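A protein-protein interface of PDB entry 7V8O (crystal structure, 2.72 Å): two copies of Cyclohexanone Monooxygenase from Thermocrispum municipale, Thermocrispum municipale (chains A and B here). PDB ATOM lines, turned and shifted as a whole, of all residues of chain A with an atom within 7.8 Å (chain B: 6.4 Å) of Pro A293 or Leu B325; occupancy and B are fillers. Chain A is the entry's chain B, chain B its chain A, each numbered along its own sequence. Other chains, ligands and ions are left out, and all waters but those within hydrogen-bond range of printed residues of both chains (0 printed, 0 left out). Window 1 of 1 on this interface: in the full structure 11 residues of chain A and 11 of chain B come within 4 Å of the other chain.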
ATOM      1  N   MET A 258       6.135  18.269  35.165  1.00  0.00           N
ATOM      2  CA  MET A 258       4.871  17.484  35.196  1.00  0.00           C
ATOM      3  C   MET A 258       5.153  16.023  35.590  1.00  0.00           C
ATOM      4  O   MET A 258       4.228  15.206  35.499  1.00  0.00           O
ATOM      5  CB  MET A 258       4.185  17.537  33.829  1.00  0.00           C
ATOM      6  CG  MET A 258       4.086  18.945  33.243  1.00  0.00           C
ATOM      7  SD  MET A 258       3.348  20.190  34.352  1.00  0.00           S
ATOM      8  CE  MET A 258       1.832  19.365  34.837  1.00  0.00           C
ATOM      9  N   ASP A 288      12.421  22.166  32.121  1.00  0.00           N
ATOM     10  CA  ASP A 288      11.663  22.137  30.838  1.00  0.00           C
ATOM     11  C   ASP A 288      10.587  23.229  30.810  1.00  0.00           C
ATOM     12  O   ASP A 288       9.607  23.052  30.062  1.00  0.00           O
ATOM     13  CB  ASP A 288      11.068  20.743  30.588  1.00  0.00           C
ATOM     14  CG  ASP A 288      10.021  20.294  31.596  1.00  0.00           C
ATOM     15  OD1 ASP A 288       9.827  20.995  32.607  1.00  0.00           O
ATOM     16  OD2 ASP A 288       9.413  19.239  31.365  1.00  0.00           O
ATOM     17  N   ILE A 289      10.773  24.331  31.539  1.00  0.00           N
ATOM     18  CA  ILE A 289       9.801  25.469  31.565  1.00  0.00           C
ATOM     19  C   ILE A 289       9.782  26.158  30.193  1.00  0.00           C
ATOM     20  O   ILE A 289       8.712  26.666  29.808  1.00  0.00           O
ATOM     21  CB  ILE A 289      10.114  26.465  32.701  1.00  0.00           C
ATOM     22  CG1 ILE A 289      10.085  25.796  34.077  1.00  0.00           C
ATOM     23  CG2 ILE A 289       9.172  27.660  32.652  1.00  0.00           C
ATOM     24  CD1 ILE A 289       8.729  25.254  34.469  1.00  0.00           C
ATOM     25  N   ALA A 290      10.909  26.173  29.478  1.00  0.00           N
ATOM     26  CA  ALA A 290      11.070  26.899  28.198  1.00  0.00           C
ATOM     27  C   ALA A 290      10.890  25.960  26.997  1.00  0.00           C
ATOM     28  O   ALA A 290      10.836  26.482  25.866  1.00  0.00           O
ATOM     29  CB  ALA A 290      12.420  27.570  28.167  1.00  0.00           C
ATOM     30  N   THR A 291      10.809  24.642  27.216  1.00  0.00           N
ATOM     31  CA  THR A 291      10.760  23.612  26.139  1.00  0.00           C
ATOM     32  C   THR A 291       9.373  22.960  26.073  1.00  0.00           C
ATOM     33  O   THR A 291       8.850  22.816  24.955  1.00  0.00           O
ATOM     34  CB  THR A 291      11.840  22.541  26.334  1.00  0.00           C
ATOM     35  OG1 THR A 291      11.581  21.857  27.561  1.00  0.00           O
ATOM     36  CG2 THR A 291      13.240  23.121  26.331  1.00  0.00           C
ATOM     37  N   ASN A 292       8.822  22.560  27.223  1.00  0.00           N
ATOM     38  CA  ASN A 292       7.545  21.807  27.334  1.00  0.00           C
ATOM     39  C   ASN A 292       6.417  22.778  27.678  1.00  0.00           C
ATOM     40  O   ASN A 292       6.497  23.467  28.694  1.00  0.00           O
ATOM     41  CB  ASN A 292       7.668  20.684  28.365  1.00  0.00           C
ATOM     42  CG  ASN A 292       6.332  20.138  28.813  1.00  0.00           C
ATOM     43  OD1 ASN A 292       5.288  20.754  28.587  1.00  0.00           O
ATOM     44  ND2 ASN A 292       6.359  18.988  29.464  1.00  0.00           N
ATOM     45  N   PRO A 293       5.324  22.845  26.875  1.00  0.00           N
ATOM     46  CA  PRO A 293       4.276  23.850  27.071  1.00  0.00           C
ATOM     47  C   PRO A 293       3.416  23.635  28.326  1.00  0.00           C
ATOM     48  O   PRO A 293       3.000  24.624  28.898  1.00  0.00           O
ATOM     49  CB  PRO A 293       3.404  23.736  25.811  1.00  0.00           C
ATOM     50  CG  PRO A 293       4.224  22.907  24.840  1.00  0.00           C
ATOM     51  CD  PRO A 293       5.043  21.988  25.712  1.00  0.00           C
ATOM     52  N   GLU A 294       3.159  22.380  28.710  1.00  0.00           N
ATOM     53  CA  GLU A 294       2.423  22.033  29.961  1.00  0.00           C
ATOM     54  C   GLU A 294       3.169  22.679  31.141  1.00  0.00           C
ATOM     55  O   GLU A 294       2.528  23.382  31.961  1.00  0.00           O
ATOM     56  CB  GLU A 294       2.316  20.510  30.113  1.00  0.00           C
ATOM     57  CG  GLU A 294       1.164  20.044  30.991  1.00  0.00           C
ATOM     58  CD  GLU A 294       0.997  18.529  31.144  1.00  0.00           C
ATOM     59  OE1 GLU A 294       1.638  17.764  30.389  1.00  0.00           O
ATOM     60  OE2 GLU A 294       0.216  18.105  32.024  1.00  0.00           O
ATOM     61  N   ALA A 295       4.489  22.475  31.193  1.00  0.00           N
ATOM     62  CA  ALA A 295       5.411  23.044  32.206  1.00  0.00           C
ATOM     63  C   ALA A 295       5.351  24.580  32.183  1.00  0.00           C
ATOM     64  O   ALA A 295       5.237  25.182  33.268  1.00  0.00           O
ATOM     65  CB  ALA A 295       6.811  22.537  31.954  1.00  0.00           C
ATOM     66  N   ASN A 296       5.424  25.185  30.992  1.00  0.00           N
ATOM     67  CA  ASN A 296       5.406  26.660  30.790  1.00  0.00           C
ATOM     68  C   ASN A 296       4.102  27.254  31.331  1.00  0.00           C
ATOM     69  O   ASN A 296       4.162  28.358  31.881  1.00  0.00           O
ATOM     70  CB  ASN A 296       5.558  27.051  29.319  1.00  0.00           C
ATOM     71  CG  ASN A 296       5.854  28.526  29.138  1.00  0.00           C
ATOM     72  OD1 ASN A 296       6.947  28.987  29.450  1.00  0.00           O
ATOM     73  ND2 ASN A 296       4.895  29.268  28.611  1.00  0.00           N
ATOM     74  N   ALA A 297       2.972  26.560  31.151  1.00  0.00           N
ATOM     75  CA  ALA A 297       1.628  26.996  31.598  1.00  0.00           C
ATOM     76  C   ALA A 297       1.555  26.948  33.126  1.00  0.00           C
ATOM     77  O   ALA A 297       0.943  27.863  33.717  1.00  0.00           O
ATOM     78  CB  ALA A 297       0.558  26.134  30.976  1.00  0.00           C
ATOM     79  N   ALA A 298       2.143  25.919  33.739  1.00  0.00           N
ATOM     80  CA  ALA A 298       2.184  25.752  35.208  1.00  0.00           C
ATOM     81  C   ALA A 298       2.885  26.962  35.835  1.00  0.00           C
ATOM     82  O   ALA A 298       2.376  27.480  36.845  1.00  0.00           O
ATOM     83  CB  ALA A 298       2.870  24.464  35.574  1.00  0.00           C
ATOM     84  N   ALA A 299       3.998  27.403  35.242  1.00  0.00           N
ATOM     85  CA  ALA A 299       4.851  28.501  35.757  1.00  0.00           C
ATOM     86  C   ALA A 299       4.139  29.845  35.569  1.00  0.00           C
ATOM     87  O   ALA A 299       4.084  30.623  36.528  1.00  0.00           O
ATOM     88  CB  ALA A 299       6.193  28.481  35.067  1.00  0.00           C
ATOM     89  N   ALA A 300       3.607  30.101  34.374  1.00  0.00           N
ATOM     90  CA  ALA A 300       2.823  31.316  34.050  1.00  0.00           C
ATOM     91  C   ALA A 300       1.622  31.413  35.000  1.00  0.00           C
ATOM     92  O   ALA A 300       1.393  32.516  35.549  1.00  0.00           O
ATOM     93  CB  ALA A 300       2.395  31.292  32.602  1.00  0.00           C
ATOM     94  N   LEU A 325       2.683  33.217  26.116  1.00  0.00           N
ATOM     95  CA  LEU A 325       3.715  32.266  26.610  1.00  0.00           C
ATOM     96  C   LEU A 325       4.712  32.986  27.537  1.00  0.00           C
ATOM     97  O   LEU A 325       5.048  34.153  27.267  1.00  0.00           O
ATOM     98  CB  LEU A 325       4.425  31.646  25.405  1.00  0.00           C
ATOM     99  CG  LEU A 325       3.560  30.777  24.492  1.00  0.00           C
ATOM    100  CD1 LEU A 325       4.384  30.223  23.339  1.00  0.00           C
ATOM    101  CD2 LEU A 325       2.905  29.641  25.262  1.00  0.00           C
ATOM    102  N   LEU A 485      10.455  27.216  23.376  1.00  0.00           N
ATOM    103  CA  LEU A 485       9.268  28.095  23.237  1.00  0.00           C
ATOM    104  C   LEU A 485       9.711  29.543  22.986  1.00  0.00           C
ATOM    105  O   LEU A 485       8.817  30.403  22.867  1.00  0.00           O
ATOM    106  CB  LEU A 485       8.427  28.020  24.514  1.00  0.00           C
ATOM    107  CG  LEU A 485       7.771  26.678  24.835  1.00  0.00           C
ATOM    108  CD1 LEU A 485       6.896  26.804  26.077  1.00  0.00           C
ATOM    109  CD2 LEU A 485       6.950  26.166  23.658  1.00  0.00           C
ATOM    110  N   TYR B 213     -11.908  23.831  30.085  1.00  0.00           N
ATOM    111  CA  TYR B 213     -12.229  24.952  29.169  1.00  0.00           C
ATOM    112  C   TYR B 213     -13.546  24.675  28.431  1.00  0.00           C
ATOM    113  O   TYR B 213     -13.509  24.304  27.236  1.00  0.00           O
ATOM    114  CB  TYR B 213     -11.063  25.156  28.199  1.00  0.00           C
ATOM    115  CG  TYR B 213      -9.777  25.639  28.824  1.00  0.00           C
ATOM    116  CD1 TYR B 213      -9.534  26.995  28.988  1.00  0.00           C
ATOM    117  CD2 TYR B 213      -8.790  24.751  29.222  1.00  0.00           C
ATOM    118  CE1 TYR B 213      -8.349  27.458  29.540  1.00  0.00           C
ATOM    119  CE2 TYR B 213      -7.600  25.198  29.782  1.00  0.00           C
ATOM    120  CZ  TYR B 213      -7.376  26.556  29.934  1.00  0.00           C
ATOM    121  OH  TYR B 213      -6.212  27.021  30.472  1.00  0.00           O
ATOM    122  N   PRO B 293       1.621  26.137  20.720  1.00  0.00           N
ATOM    123  CA  PRO B 293       1.402  26.637  22.078  1.00  0.00           C
ATOM    124  C   PRO B 293       0.929  28.095  22.150  1.00  0.00           C
ATOM    125  O   PRO B 293       0.129  28.387  23.000  1.00  0.00           O
ATOM    126  CB  PRO B 293       2.786  26.514  22.730  1.00  0.00           C
ATOM    127  CG  PRO B 293       3.434  25.366  21.993  1.00  0.00           C
ATOM    128  CD  PRO B 293       2.957  25.537  20.564  1.00  0.00           C
ATOM    129  N   ASN B 296      -2.637  28.192  21.295  1.00  0.00           N
ATOM    130  CA  ASN B 296      -3.333  27.540  22.432  1.00  0.00           C
ATOM    131  C   ASN B 296      -3.548  28.565  23.550  1.00  0.00           C
ATOM    132  O   ASN B 296      -4.641  28.570  24.144  1.00  0.00           O
ATOM    133  CB  ASN B 296      -2.570  26.314  22.921  1.00  0.00           C
ATOM    134  CG  ASN B 296      -3.454  25.374  23.704  1.00  0.00           C
ATOM    135  OD1 ASN B 296      -4.219  24.611  23.125  1.00  0.00           O
ATOM    136  ND2 ASN B 296      -3.356  25.424  25.020  1.00  0.00           N
ATOM    137  N   ALA B 300      -7.129  29.618  25.147  1.00  0.00           N
ATOM    138  CA  ALA B 300      -7.353  29.475  26.604  1.00  0.00           C
ATOM    139  C   ALA B 300      -7.693  30.842  27.214  1.00  0.00           C
ATOM    140  O   ALA B 300      -8.649  30.919  28.008  1.00  0.00           O
ATOM    141  CB  ALA B 300      -6.138  28.867  27.252  1.00  0.00           C
ATOM    142  N   THR B 323      -5.969  26.575  34.145  1.00  0.00           N
ATOM    143  CA  THR B 323      -4.626  27.178  33.916  1.00  0.00           C
ATOM    144  C   THR B 323      -3.703  26.230  33.139  1.00  0.00           C
ATOM    145  O   THR B 323      -2.611  26.686  32.767  1.00  0.00           O
ATOM    146  CB  THR B 323      -3.965  27.565  35.249  1.00  0.00           C
ATOM    147  OG1 THR B 323      -4.041  26.456  36.149  1.00  0.00           O
ATOM    148  CG2 THR B 323      -4.591  28.780  35.897  1.00  0.00           C
ATOM    149  N   ASP B 324      -4.109  24.975  32.908  1.00  0.00           N
ATOM    150  CA  ASP B 324      -3.333  23.953  32.145  1.00  0.00           C
ATOM    151  C   ASP B 324      -3.510  24.232  30.643  1.00  0.00           C
ATOM    152  O   ASP B 324      -3.982  25.328  30.304  1.00  0.00           O
ATOM    153  CB  ASP B 324      -3.732  22.535  32.571  1.00  0.00           C
ATOM    154  CG  ASP B 324      -5.229  22.322  32.739  1.00  0.00           C
ATOM    155  OD1 ASP B 324      -6.000  23.013  32.046  1.00  0.00           O
ATOM    156  OD2 ASP B 324      -5.612  21.480  33.578  1.00  0.00           O
ATOM    157  N   LEU B 325      -3.129  23.299  29.764  1.00  0.00           N
ATOM    158  CA  LEU B 325      -3.365  23.419  28.298  1.00  0.00           C
ATOM    159  C   LEU B 325      -4.834  23.089  27.983  1.00  0.00           C
ATOM    160  O   LEU B 325      -5.418  22.226  28.674  1.00  0.00           O
ATOM    161  CB  LEU B 325      -2.412  22.491  27.534  1.00  0.00           C
ATOM    162  CG  LEU B 325      -0.918  22.765  27.722  1.00  0.00           C
ATOM    163  CD1 LEU B 325      -0.073  21.645  27.125  1.00  0.00           C
ATOM    164  CD2 LEU B 325      -0.535  24.103  27.111  1.00  0.00           C
ATOM    165  N   TYR B 326      -5.402  23.790  26.995  1.00  0.00           N
ATOM    166  CA  TYR B 326      -6.676  23.464  26.302  1.00  0.00           C
ATOM    167  C   TYR B 326      -6.388  22.302  25.345  1.00  0.00           C
ATOM    168  O   TYR B 326      -6.327  22.518  24.114  1.00  0.00           O
ATOM    169  CB  TYR B 326      -7.227  24.701  25.584  1.00  0.00           C
ATOM    170  CG  TYR B 326      -8.573  24.540  24.915  1.00  0.00           C
ATOM    171  CD1 TYR B 326      -9.608  23.864  25.532  1.00  0.00           C
ATOM    172  CD2 TYR B 326      -8.831  25.115  23.680  1.00  0.00           C
ATOM    173  CE1 TYR B 326     -10.847  23.726  24.928  1.00  0.00           C
ATOM    174  CE2 TYR B 326     -10.065  24.993  23.059  1.00  0.00           C
ATOM    175  CZ  TYR B 326     -11.083  24.297  23.689  1.00  0.00           C
ATOM    176  OH  TYR B 326     -12.308  24.163  23.097  1.00  0.00           O
ATOM    177  N   ALA B 327      -6.157  21.112  25.912  1.00  0.00           N
ATOM    178  CA  ALA B 327      -5.745  19.903  25.159  1.00  0.00           C
ATOM    179  C   ALA B 327      -6.414  18.632  25.705  1.00  0.00           C
ATOM    180  O   ALA B 327      -5.961  17.533  25.320  1.00  0.00           O
ATOM    181  CB  ALA B 327      -4.240  19.799  25.179  1.00  0.00           C
ATOM    182  N   LYS B 328      -7.447  18.765  26.548  1.00  0.00           N
ATOM    183  CA  LYS B 328      -8.439  17.685  26.825  1.00  0.00           C
ATOM    184  C   LYS B 328      -9.496  17.726  25.713  1.00  0.00           C
ATOM    185  O   LYS B 328      -9.460  18.664  24.897  1.00  0.00           O
ATOM    186  CB  LYS B 328      -9.079  17.859  28.204  1.00  0.00           C
ATOM    187  CG  LYS B 328      -8.100  18.091  29.346  1.00  0.00           C
ATOM    188  CD  LYS B 328      -8.737  17.978  30.716  1.00  0.00           C
ATOM    189  CE  LYS B 328      -7.728  17.901  31.842  1.00  0.00           C
ATOM    190  NZ  LYS B 328      -6.942  19.153  31.968  1.00  0.00           N
ATOM    191  N   LEU B 485      -0.435  18.934  21.176  1.00  0.00           N
ATOM    192  CA  LEU B 485      -0.437  19.258  22.626  1.00  0.00           C
ATOM    193  C   LEU B 485      -1.236  18.203  23.403  1.00  0.00           C
ATOM    194  O   LEU B 485      -1.146  18.212  24.636  1.00  0.00           O
ATOM    195  CB  LEU B 485      -1.022  20.659  22.826  1.00  0.00           C
ATOM    196  CG  LEU B 485      -0.216  21.803  22.207  1.00  0.00           C
ATOM    197  CD1 LEU B 485      -0.971  23.119  22.312  1.00  0.00           C
ATOM    198  CD2 LEU B 485       1.157  21.921  22.855  1.00  0.00           C
ATOM    199  N   LYS B 488       0.218  16.060  26.434  1.00  0.00           N
ATOM    200  CA  LYS B 488       0.558  16.840  27.652  1.00  0.00           C
ATOM    201  C   LYS B 488      -0.731  17.374  28.295  1.00  0.00           C
ATOM    202  O   LYS B 488      -0.737  18.546  28.724  1.00  0.00           O
ATOM    203  CB  LYS B 488       1.523  17.965  27.264  1.00  0.00           C
ATOM    204  CG  LYS B 488       2.742  17.525  26.460  1.00  0.00           C
ATOM    205  CD  LYS B 488       3.527  18.679  25.873  1.00  0.00           C
ATOM    206  CE  LYS B 488       4.212  18.334  24.568  1.00  0.00           C
ATOM    207  NZ  LYS B 488       5.011  17.092  24.687  1.00  0.00           N
ATOM    208  N   ALA B 489      -1.778  16.547  28.367  1.00  0.00           N
ATOM    209  CA  ALA B 489      -3.130  16.924  28.847  1.00  0.00           C
ATOM    210  C   ALA B 489      -3.382  16.346  30.244  1.00  0.00           C
ATOM    211  O   ALA B 489      -3.913  17.081  31.108  1.00  0.00           O
ATOM    212  CB  ALA B 489      -4.171  16.446  27.866  1.00  0.00           C
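Pro A293 touches its own counterpart, Pro B293.
Pro A293 touches Leu B325, and with the chains exchanged Leu A325 touches Pro B293.
Pro A293 touches Leu B485, and with the chains exchanged Leu A485 touches Pro B293.
5 positions are printed for both chains.
Of the 10 pairs that touch across the chains among the printed residues, 5 have their exchanged pair printed and touching as well.
Of the printed residues of chain B, Pro A293 touches Pro B293 (3.8 Å), Leu B325 (3.995 Å), Leu B485 (3.8 Å) and Lys B488 (3.6 Å).
Printed residues of chain A within 4 Å of Leu B325: Pro A293 and Glu A294.
Of the printed residues of chain B, Leu A325 touches Pro B293 (3.8 Å).
Printed residues of chain B within 4 Å of Leu A485: Pro B293 (3.97 Å).
Of the printed residues of chain A, Lys B488 touches Asn A292, Pro A293 and Glu A294.
Of the printed residues of chain B, Ala A297 touches Thr B323 (3.7 Å).
Of the printed residues of chain A, Leu B485 touches Pro A293 (3.8 Å).
Asn B296 touches none of the printed residues of chain A.
The nearest printed residue of chain B that does not touch Glu A294 is Ala B489 (4.2 Å).
The side-chain carboxylate of Glu A294 sits close to the backbone carbonyl oxygen of Lys B488 (3.0 Å).
Of the 16 printed residues of chain A, 6 touch a printed residue of chain B.
Printed residues of chain B that touch a printed residue of chain A: Pro B293, Thr B323, Leu B325, Leu B485 and Lys B488.
Hydrophobic or aromatic side chains of chain B that line the printed part of chain A: Pro B293, Leu B325 and Leu B485.
Among the printed residues, no Asp or Glu carboxylate lies within 4 Å of a Lys or Arg side-chain nitrogen of the other chain.
Lys B488 touches Asn A292 (CD to OD1, 3.8 Å).
Pro A293 touches Pro B293.
O of Pro A293 touches CD2 of Leu B325, at 3.995 Å.
CD2 of Leu B485 touches CG of Pro A293, 3.8 Å away.
Pro A293 touches Lys B488.
Glu A294 touches Leu B325.
Thr B323 touches Ala A297 (O to CB, 3.7 Å).
Pro B293 touches Leu A325.
Pro B293 touches Leu A485.
The backbone carbonyl oxygen (O) of Ala A290 lies within hydrogen-bond range of the backbone NH (N) of Leu A485 (2.6 Å).
OD1 of Asn A292 sits at hydrogen-bond distance from N of Glu A294 (2.7 Å).
The side-chain amide oxygen (OD1) of Asn A292 sits at hydrogen-bond distance from the backbone NH (N) of Ala A295 (3.2 Å).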
